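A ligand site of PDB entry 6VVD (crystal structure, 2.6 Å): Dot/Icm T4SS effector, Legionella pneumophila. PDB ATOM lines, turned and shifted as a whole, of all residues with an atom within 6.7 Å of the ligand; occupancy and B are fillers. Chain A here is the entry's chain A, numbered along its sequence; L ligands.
An oxygen (O23) of the ligand lies within hydrogen-bond range of the side-chain hydroxyl (OG) of Ser 66, at 2.4 Å. O23 of the ligand is in salt-bridge range of NH1 of Arg 42 (2.6 Å). NZ of Lys 68 lies within salt-bridge range of O14 of the ligand (2.6 Å). The side-chain amino group of Lys 99 lies within salt-bridge range of an oxygen (O3) of the ligand, at 2.6 Å. A ring nitrogen (ND1) of His 29 lies within hydrogen-bond range of an oxygen (O18) of the ligand (2.6 Å). The side-chain amino group (NZ) of Lys 148 is in salt-bridge range of an oxygen (O12) of the ligand, 2.7 Å away. An oxygen (O20) of the ligand is in hydrogen-bond range of the side-chain hydroxyl (OH) of Tyr 30, 2.7 Å away. The backbone NH (N) of His 67 lies within hydrogen-bond range of an oxygen (O2) of the ligand (2.9 Å). O of His 67 lies close to O4 of the ligand. ND2 of Asn 146 is in hydrogen-bond range of O19 of the ligand. NZ of Lys 103 lies within salt-bridge range of O3 of the ligand (3.1 Å). The indole nitrogen of Trp 64 sits at hydrogen-bond distance from an oxygen (O22) of the ligand, 3.1 Å away.
O of Thr 24 lies within hydrogen-bond range of N of Arg 42, at 2.8 Å. OD1 of Asn 146 sits at hydrogen-bond distance from N of Lys 148, 3.3 Å away. OH of Tyr 30 sits at hydrogen-bond distance from ND2 of Asn 146 (3.2 Å). ND1 of His 67 is in hydrogen-bond range of OG1 of Thr 100, at 3.5 Å. The backbone NH (N) of Asn 146 sits at hydrogen-bond distance from the backbone carbonyl oxygen (O) of Tyr 154, 2.8 Å away. The side-chain hydroxyl of Tyr 156 lies close to the side-chain amino group of Lys 103. The backbone NH (N) of Val 47 is in hydrogen-bond range of the backbone carbonyl oxygen (O) of Trp 64 (2.9 Å). The backbone NH of Leu 26 lies within hydrogen-bond range of the backbone carbonyl oxygen of Ile 40 (2.8 Å).
Merely in contact with the ligand: Leu 26 (3.996 Å), Val 47 (3.4 Å), Thr 100 (3.4 Å) and Tyr 154 (3.8 Å). 15 residues have an atom within 4 Å of the ligand: Leu 26, His 29, Tyr 30, Arg 42, Val 47, Trp 64, Ser 66, His 67, Lys 68, Lys 99, Thr 100, Lys 103, Asn 146, Lys 148 and Tyr 154. The nearest printed residue that does not touch the ligand is Lys 65 (4.2 Å).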
ATOM      1  N   THR A  24      -0.610  14.275  -8.000  1.00  0.00           N
ATOM      2  CA  THR A  24      -0.687  14.593  -6.579  1.00  0.00           C
ATOM      3  C   THR A  24      -1.771  13.748  -5.916  1.00  0.00           C
ATOM      4  O   THR A  24      -2.934  13.770  -6.348  1.00  0.00           O
ATOM      5  CB  THR A  24      -0.976  16.083  -6.386  1.00  0.00           C
ATOM      6  OG1 THR A  24      -0.053  16.856  -7.159  1.00  0.00           O
ATOM      7  CG2 THR A  24      -0.848  16.465  -4.912  1.00  0.00           C
ATOM      8  N   LEU A  26      -4.466  12.904  -3.386  1.00  0.00           N
ATOM      9  CA  LEU A  26      -5.403  13.603  -2.511  1.00  0.00           C
ATOM     10  C   LEU A  26      -6.273  12.646  -1.715  1.00  0.00           C
ATOM     11  O   LEU A  26      -7.231  13.084  -1.064  1.00  0.00           O
ATOM     12  CB  LEU A  26      -6.289  14.532  -3.348  1.00  0.00           C
ATOM     13  CG  LEU A  26      -5.569  15.497  -4.298  1.00  0.00           C
ATOM     14  CD1 LEU A  26      -6.575  16.236  -5.180  1.00  0.00           C
ATOM     15  CD2 LEU A  26      -4.701  16.466  -3.519  1.00  0.00           C
ATOM     16  N   HIS A  29      -7.997  13.124   1.845  1.00  0.00           N
ATOM     17  CA  HIS A  29      -8.976  14.195   1.992  1.00  0.00           C
ATOM     18  C   HIS A  29     -10.389  13.757   1.632  1.00  0.00           C
ATOM     19  O   HIS A  29     -11.325  14.543   1.808  1.00  0.00           O
ATOM     20  CB  HIS A  29      -8.588  15.401   1.132  1.00  0.00           C
ATOM     21  CG  HIS A  29      -7.293  16.045   1.543  1.00  0.00           C
ATOM     22  ND1 HIS A  29      -6.556  16.827   0.678  1.00  0.00           N
ATOM     23  CD2 HIS A  29      -6.617  16.011   2.702  1.00  0.00           C
ATOM     24  CE1 HIS A  29      -5.475  17.265   1.307  1.00  0.00           C
ATOM     25  NE2 HIS A  29      -5.483  16.778   2.536  1.00  0.00           N
ATOM     26  N   TYR A  30     -10.570  12.526   1.141  1.00  0.00           N
ATOM     27  CA  TYR A  30     -11.871  12.085   0.648  1.00  0.00           C
ATOM     28  C   TYR A  30     -12.227  10.691   1.120  1.00  0.00           C
ATOM     29  O   TYR A  30     -13.360  10.443   1.553  1.00  0.00           O
ATOM     30  CB  TYR A  30     -11.894  12.140  -0.882  1.00  0.00           C
ATOM     31  CG  TYR A  30     -11.726  13.529  -1.450  1.00  0.00           C
ATOM     32  CD1 TYR A  30     -12.810  14.364  -1.608  1.00  0.00           C
ATOM     33  CD2 TYR A  30     -10.475  14.004  -1.807  1.00  0.00           C
ATOM     34  CE1 TYR A  30     -12.676  15.635  -2.115  1.00  0.00           C
ATOM     35  CE2 TYR A  30     -10.319  15.279  -2.318  1.00  0.00           C
ATOM     36  CZ  TYR A  30     -11.419  16.086  -2.469  1.00  0.00           C
ATOM     37  OH  TYR A  30     -11.285  17.357  -2.976  1.00  0.00           O
ATOM     38  N   ILE A  40      -7.529   9.059  -5.052  1.00  0.00           N
ATOM     39  CA  ILE A  40      -7.864  10.347  -5.646  1.00  0.00           C
ATOM     40  C   ILE A  40      -6.570  11.044  -6.038  1.00  0.00           C
ATOM     41  O   ILE A  40      -5.684  11.217  -5.201  1.00  0.00           O
ATOM     42  CB  ILE A  40      -8.673  11.228  -4.666  1.00  0.00           C
ATOM     43  CG1 ILE A  40      -9.914  10.482  -4.162  1.00  0.00           C
ATOM     44  CG2 ILE A  40      -9.085  12.531  -5.334  1.00  0.00           C
ATOM     45  CD1 ILE A  40     -10.865  10.038  -5.247  1.00  0.00           C
ATOM     46  N   ARG A  42      -4.639  14.255  -8.525  1.00  0.00           N
ATOM     47  CA  ARG A  42      -4.656  15.465  -9.331  1.00  0.00           C
ATOM     48  C   ARG A  42      -3.602  15.348 -10.417  1.00  0.00           C
ATOM     49  O   ARG A  42      -2.469  14.929 -10.159  1.00  0.00           O
ATOM     50  CB  ARG A  42      -4.370  16.688  -8.464  1.00  0.00           C
ATOM     51  CG  ARG A  42      -4.683  18.011  -9.128  1.00  0.00           C
ATOM     52  CD  ARG A  42      -4.981  19.049  -8.056  1.00  0.00           C
ATOM     53  NE  ARG A  42      -3.938  19.059  -7.034  1.00  0.00           N
ATOM     54  CZ  ARG A  42      -4.117  19.406  -5.762  1.00  0.00           C
ATOM     55  NH1 ARG A  42      -5.311  19.765  -5.333  1.00  0.00           N
ATOM     56  NH2 ARG A  42      -3.097  19.388  -4.924  1.00  0.00           N
ATOM     57  N   VAL A  47      -8.872  16.408 -11.316  1.00  0.00           N
ATOM     58  CA  VAL A  47      -8.937  15.465 -10.206  1.00  0.00           C
ATOM     59  C   VAL A  47      -9.576  14.190 -10.718  1.00  0.00           C
ATOM     60  O   VAL A  47     -10.637  14.220 -11.353  1.00  0.00           O
ATOM     61  CB  VAL A  47      -9.724  16.044  -9.016  1.00  0.00           C
ATOM     62  CG1 VAL A  47     -10.014  14.947  -8.001  1.00  0.00           C
ATOM     63  CG2 VAL A  47      -8.940  17.167  -8.366  1.00  0.00           C
ATOM     64  N   TRP A  64     -13.536  16.387 -11.597  1.00  0.00           N
ATOM     65  CA  TRP A  64     -13.680  17.819 -11.804  1.00  0.00           C
ATOM     66  C   TRP A  64     -12.313  18.406 -12.157  1.00  0.00           C
ATOM     67  O   TRP A  64     -11.289  17.729 -12.070  1.00  0.00           O
ATOM     68  CB  TRP A  64     -14.256  18.520 -10.566  1.00  0.00           C
ATOM     69  CG  TRP A  64     -13.405  18.442  -9.343  1.00  0.00           C
ATOM     70  CD1 TRP A  64     -12.267  19.153  -9.079  1.00  0.00           C
ATOM     71  CD2 TRP A  64     -13.638  17.621  -8.193  1.00  0.00           C
ATOM     72  NE1 TRP A  64     -11.771  18.815  -7.842  1.00  0.00           N
ATOM     73  CE2 TRP A  64     -12.590  17.881  -7.275  1.00  0.00           C
ATOM     74  CE3 TRP A  64     -14.616  16.689  -7.842  1.00  0.00           C
ATOM     75  CZ2 TRP A  64     -12.503  17.238  -6.045  1.00  0.00           C
ATOM     76  CZ3 TRP A  64     -14.524  16.055  -6.622  1.00  0.00           C
ATOM     77  CH2 TRP A  64     -13.474  16.329  -5.733  1.00  0.00           C
ATOM     78  N   LYS A  65     -12.328  19.679 -12.565  1.00  0.00           N
ATOM     79  CA  LYS A  65     -11.123  20.410 -12.948  1.00  0.00           C
ATOM     80  C   LYS A  65     -10.612  21.220 -11.756  1.00  0.00           C
ATOM     81  O   LYS A  65     -11.378  21.660 -10.906  1.00  0.00           O
ATOM     82  CB  LYS A  65     -11.428  21.323 -14.139  1.00  0.00           C
ATOM     83  CG  LYS A  65     -11.853  20.533 -15.377  1.00  0.00           C
ATOM     84  CD  LYS A  65     -12.475  21.404 -16.473  1.00  0.00           C
ATOM     85  CE  LYS A  65     -12.747  20.576 -17.726  1.00  0.00           C
ATOM     86  NZ  LYS A  65     -13.725  21.210 -18.653  1.00  0.00           N
ATOM     87  N   SER A  66      -9.287  21.399 -11.711  1.00  0.00           N
ATOM     88  CA  SER A  66      -8.632  21.985 -10.550  1.00  0.00           C
ATOM     89  C   SER A  66      -7.900  23.270 -10.917  1.00  0.00           C
ATOM     90  O   SER A  66      -7.598  23.539 -12.083  1.00  0.00           O
ATOM     91  CB  SER A  66      -7.626  20.990  -9.928  1.00  0.00           C
ATOM     92  OG  SER A  66      -7.079  21.504  -8.729  1.00  0.00           O
ATOM     93  N   HIS A  67      -7.616  24.073  -9.886  1.00  0.00           N
ATOM     94  CA  HIS A  67      -6.923  25.351 -10.033  1.00  0.00           C
ATOM     95  C   HIS A  67      -5.933  25.532  -8.889  1.00  0.00           C
ATOM     96  O   HIS A  67      -5.876  26.586  -8.237  1.00  0.00           O
ATOM     97  CB  HIS A  67      -7.925  26.513 -10.069  1.00  0.00           C
ATOM     98  CG  HIS A  67      -8.561  26.734 -11.400  1.00  0.00           C
ATOM     99  ND1 HIS A  67      -9.849  27.211 -11.543  1.00  0.00           N
ATOM    100  CD2 HIS A  67      -8.089  26.563 -12.661  1.00  0.00           C
ATOM    101  CE1 HIS A  67     -10.140  27.312 -12.827  1.00  0.00           C
ATOM    102  NE2 HIS A  67      -9.094  26.923 -13.528  1.00  0.00           N
ATOM    103  N   LYS A  68      -5.141  24.507  -8.619  1.00  0.00           N
ATOM    104  CA  LYS A  68      -4.157  24.561  -7.529  1.00  0.00           C
ATOM    105  C   LYS A  68      -3.033  25.532  -7.871  1.00  0.00           C
ATOM    106  O   LYS A  68      -2.449  25.469  -8.949  1.00  0.00           O
ATOM    107  CB  LYS A  68      -3.600  23.169  -7.249  1.00  0.00           C
ATOM    108  CG  LYS A  68      -2.493  23.111  -6.208  1.00  0.00           C
ATOM    109  CD  LYS A  68      -3.032  23.227  -4.786  1.00  0.00           C
ATOM    110  CE  LYS A  68      -2.091  22.528  -3.804  1.00  0.00           C
ATOM    111  NZ  LYS A  68      -2.298  22.966  -2.395  1.00  0.00           N
ATOM    112  N   TYR A  85     -17.314  33.594  -1.062  1.00  0.00           N
ATOM    113  CA  TYR A  85     -17.510  33.141  -2.434  1.00  0.00           C
ATOM    114  C   TYR A  85     -18.918  33.515  -2.905  1.00  0.00           C
ATOM    115  O   TYR A  85     -19.827  33.746  -2.098  1.00  0.00           O
ATOM    116  CB  TYR A  85     -17.317  31.632  -2.567  1.00  0.00           C
ATOM    117  CG  TYR A  85     -15.975  31.129  -2.094  1.00  0.00           C
ATOM    118  CD1 TYR A  85     -14.828  31.297  -2.859  1.00  0.00           C
ATOM    119  CD2 TYR A  85     -15.863  30.470  -0.874  1.00  0.00           C
ATOM    120  CE1 TYR A  85     -13.607  30.837  -2.420  1.00  0.00           C
ATOM    121  CE2 TYR A  85     -14.635  30.000  -0.429  1.00  0.00           C
ATOM    122  CZ  TYR A  85     -13.512  30.182  -1.207  1.00  0.00           C
ATOM    123  OH  TYR A  85     -12.291  29.722  -0.768  1.00  0.00           O
ATOM    124  N   LYS A  99     -16.506  27.997  -5.797  1.00  0.00           N
ATOM    125  CA  LYS A  99     -15.119  27.995  -5.358  1.00  0.00           C
ATOM    126  C   LYS A  99     -14.204  28.468  -6.486  1.00  0.00           C
ATOM    127  O   LYS A  99     -13.397  29.379  -6.303  1.00  0.00           O
ATOM    128  CB  LYS A  99     -14.719  26.600  -4.893  1.00  0.00           C
ATOM    129  CG  LYS A  99     -13.283  26.470  -4.384  1.00  0.00           C
ATOM    130  CD  LYS A  99     -13.072  27.247  -3.088  1.00  0.00           C
ATOM    131  CE  LYS A  99     -11.770  26.855  -2.395  1.00  0.00           C
ATOM    132  NZ  LYS A  99     -10.738  26.342  -3.349  1.00  0.00           N
ATOM    133  N   THR A 100     -14.329  27.863  -7.661  1.00  0.00           N
ATOM    134  CA  THR A 100     -13.707  28.354  -8.875  1.00  0.00           C
ATOM    135  C   THR A 100     -14.735  28.306  -9.995  1.00  0.00           C
ATOM    136  O   THR A 100     -15.850  27.811  -9.813  1.00  0.00           O
ATOM    137  CB  THR A 100     -12.465  27.540  -9.247  1.00  0.00           C
ATOM    138  OG1 THR A 100     -12.851  26.402 -10.026  1.00  0.00           O
ATOM    139  CG2 THR A 100     -11.738  27.064  -7.995  1.00  0.00           C
ATOM    140  N   LYS A 103     -15.783  24.656 -10.817  1.00  0.00           N
ATOM    141  CA  LYS A 103     -16.048  23.760  -9.700  1.00  0.00           C
ATOM    142  C   LYS A 103     -16.980  24.423  -8.708  1.00  0.00           C
ATOM    143  O   LYS A 103     -16.720  25.534  -8.258  1.00  0.00           O
ATOM    144  CB  LYS A 103     -14.732  23.366  -9.011  1.00  0.00           C
ATOM    145  CG  LYS A 103     -14.928  22.719  -7.653  1.00  0.00           C
ATOM    146  CD  LYS A 103     -13.667  21.976  -7.225  1.00  0.00           C
ATOM    147  CE  LYS A 103     -12.536  22.930  -6.862  1.00  0.00           C
ATOM    148  NZ  LYS A 103     -12.109  22.754  -5.448  1.00  0.00           N
ATOM    149  N   ASN A 146     -15.351  16.536   0.646  1.00  0.00           N
ATOM    150  CA  ASN A 146     -14.034  16.827   1.201  1.00  0.00           C
ATOM    151  C   ASN A 146     -14.120  16.766   2.713  1.00  0.00           C
ATOM    152  O   ASN A 146     -14.875  17.530   3.330  1.00  0.00           O
ATOM    153  CB  ASN A 146     -13.547  18.198   0.734  1.00  0.00           C
ATOM    154  CG  ASN A 146     -12.096  18.454   1.057  1.00  0.00           C
ATOM    155  OD1 ASN A 146     -11.722  18.519   2.229  1.00  0.00           O
ATOM    156  ND2 ASN A 146     -11.272  18.606   0.023  1.00  0.00           N
ATOM    157  N   LYS A 148     -11.217  16.640   4.854  1.00  0.00           N
ATOM    158  CA  LYS A 148      -9.927  16.888   5.489  1.00  0.00           C
ATOM    159  C   LYS A 148     -10.093  17.711   6.758  1.00  0.00           C
ATOM    160  O   LYS A 148      -9.281  17.575   7.689  1.00  0.00           O
ATOM    161  CB  LYS A 148      -8.971  17.576   4.515  1.00  0.00           C
ATOM    162  CG  LYS A 148      -9.232  19.046   4.293  1.00  0.00           C
ATOM    163  CD  LYS A 148      -8.580  19.478   2.993  1.00  0.00           C
ATOM    164  CE  LYS A 148      -8.771  20.952   2.702  1.00  0.00           C
ATOM    165  NZ  LYS A 148      -8.120  21.336   1.421  1.00  0.00           N
ATOM    166  N   TYR A 154     -17.531  19.947   2.873  1.00  0.00           N
ATOM    167  CA  TYR A 154     -18.225  20.466   1.700  1.00  0.00           C
ATOM    168  C   TYR A 154     -18.094  19.462   0.570  1.00  0.00           C
ATOM    169  O   TYR A 154     -17.289  18.527   0.629  1.00  0.00           O
ATOM    170  CB  TYR A 154     -17.653  21.826   1.284  1.00  0.00           C
ATOM    171  CG  TYR A 154     -16.150  21.924   1.425  1.00  0.00           C
ATOM    172  CD1 TYR A 154     -15.554  22.228   2.641  1.00  0.00           C
ATOM    173  CD2 TYR A 154     -15.316  21.698   0.329  1.00  0.00           C
ATOM    174  CE1 TYR A 154     -14.181  22.314   2.767  1.00  0.00           C
ATOM    175  CE2 TYR A 154     -13.947  21.773   0.443  1.00  0.00           C
ATOM    176  CZ  TYR A 154     -13.379  22.080   1.666  1.00  0.00           C
ATOM    177  OH  TYR A 154     -12.004  22.164   1.770  1.00  0.00           O
ATOM    178  N   TYR A 156     -17.489  18.898  -3.461  1.00  0.00           N
ATOM    179  CA  TYR A 156     -16.994  19.421  -4.722  1.00  0.00           C
ATOM    180  C   TYR A 156     -17.644  18.696  -5.890  1.00  0.00           C
ATOM    181  O   TYR A 156     -17.930  17.492  -5.818  1.00  0.00           O
ATOM    182  CB  TYR A 156     -15.466  19.281  -4.810  1.00  0.00           C
ATOM    183  CG  TYR A 156     -14.678  20.337  -4.063  1.00  0.00           C
ATOM    184  CD1 TYR A 156     -15.104  21.654  -4.012  1.00  0.00           C
ATOM    185  CD2 TYR A 156     -13.479  20.011  -3.423  1.00  0.00           C
ATOM    186  CE1 TYR A 156     -14.381  22.611  -3.329  1.00  0.00           C
ATOM    187  CE2 TYR A 156     -12.755  20.968  -2.741  1.00  0.00           C
ATOM    188  CZ  TYR A 156     -13.208  22.269  -2.698  1.00  0.00           C
ATOM    189  OH  TYR A 156     -12.479  23.218  -2.019  1.00  0.00           O
HETATM  190  C1  LIG L   1      -8.076  23.706  -4.535  1.00  0.00           C
HETATM  191  C2  LIG L   1      -7.100  24.631  -3.803  1.00  0.00           C
HETATM  192  C3  LIG L   1      -6.927  24.247  -2.323  1.00  0.00           C
HETATM  193  C4  LIG L   1      -6.467  22.793  -2.217  1.00  0.00           C
HETATM  194  C5  LIG L   1      -7.543  21.872  -2.829  1.00  0.00           C
HETATM  195  C6  LIG L   1      -7.804  22.224  -4.297  1.00  0.00           C
HETATM  196  O1  LIG L   1      -7.981  23.942  -5.917  1.00  0.00           O
HETATM  197  P1  LIG L   1      -9.136  24.882  -6.635  1.00  0.00           P
HETATM  198  O2  LIG L   1      -9.718  24.149  -7.821  1.00  0.00           O
HETATM  199  O3  LIG L   1     -10.210  25.172  -5.614  1.00  0.00           O
HETATM  200  O4  LIG L   1      -8.535  26.169  -7.109  1.00  0.00           O
HETATM  201  O5  LIG L   1      -7.597  25.937  -3.877  1.00  0.00           O
HETATM  202  P2  LIG L   1      -6.495  27.137  -4.141  1.00  0.00           P
HETATM  203  O6  LIG L   1      -5.591  26.719  -5.284  1.00  0.00           O
HETATM  204  O7  LIG L   1      -7.180  28.430  -4.503  1.00  0.00           O
HETATM  205  O8  LIG L   1      -5.691  27.320  -2.868  1.00  0.00           O
HETATM  206  O9  LIG L   1      -8.163  24.389  -1.686  1.00  0.00           O
HETATM  207  P3  LIG L   1      -8.201  24.957  -0.134  1.00  0.00           P
HETATM  208  O10 LIG L   1      -6.802  25.350   0.271  1.00  0.00           O
HETATM  209  O11 LIG L   1      -9.123  26.149  -0.074  1.00  0.00           O
HETATM  210  O12 LIG L   1      -8.699  23.883   0.809  1.00  0.00           O
HETATM  211  O13 LIG L   1      -6.265  22.431  -0.886  1.00  0.00           O
HETATM  212  P4  LIG L   1      -4.735  21.977  -0.475  1.00  0.00           P
HETATM  213  O14 LIG L   1      -3.895  23.221  -0.359  1.00  0.00           O
HETATM  214  O15 LIG L   1      -4.175  21.072  -1.552  1.00  0.00           O
HETATM  215  O16 LIG L   1      -4.757  21.249   0.852  1.00  0.00           O
HETATM  216  O17 LIG L   1      -7.122  20.551  -2.731  1.00  0.00           O
HETATM  217  P5  LIG L   1      -8.132  19.496  -1.982  1.00  0.00           P
HETATM  218  O18 LIG L   1      -7.348  18.433  -1.252  1.00  0.00           O
HETATM  219  O19 LIG L   1      -8.988  20.241  -0.985  1.00  0.00           O
HETATM  220  O20 LIG L   1      -8.990  18.865  -3.055  1.00  0.00           O
HETATM  221  O21 LIG L   1      -8.941  21.489  -4.685  1.00  0.00           O
HETATM  222  P6  LIG L   1      -8.842  20.552  -6.023  1.00  0.00           P
HETATM  223  O22 LIG L   1      -9.764  21.074  -7.110  1.00  0.00           O
HETATM  224  O23 LIG L   1      -7.428  20.579  -6.528  1.00  0.00           O
HETATM  225  O24 LIG L   1      -9.263  19.158  -5.630  1.00  0.00           O
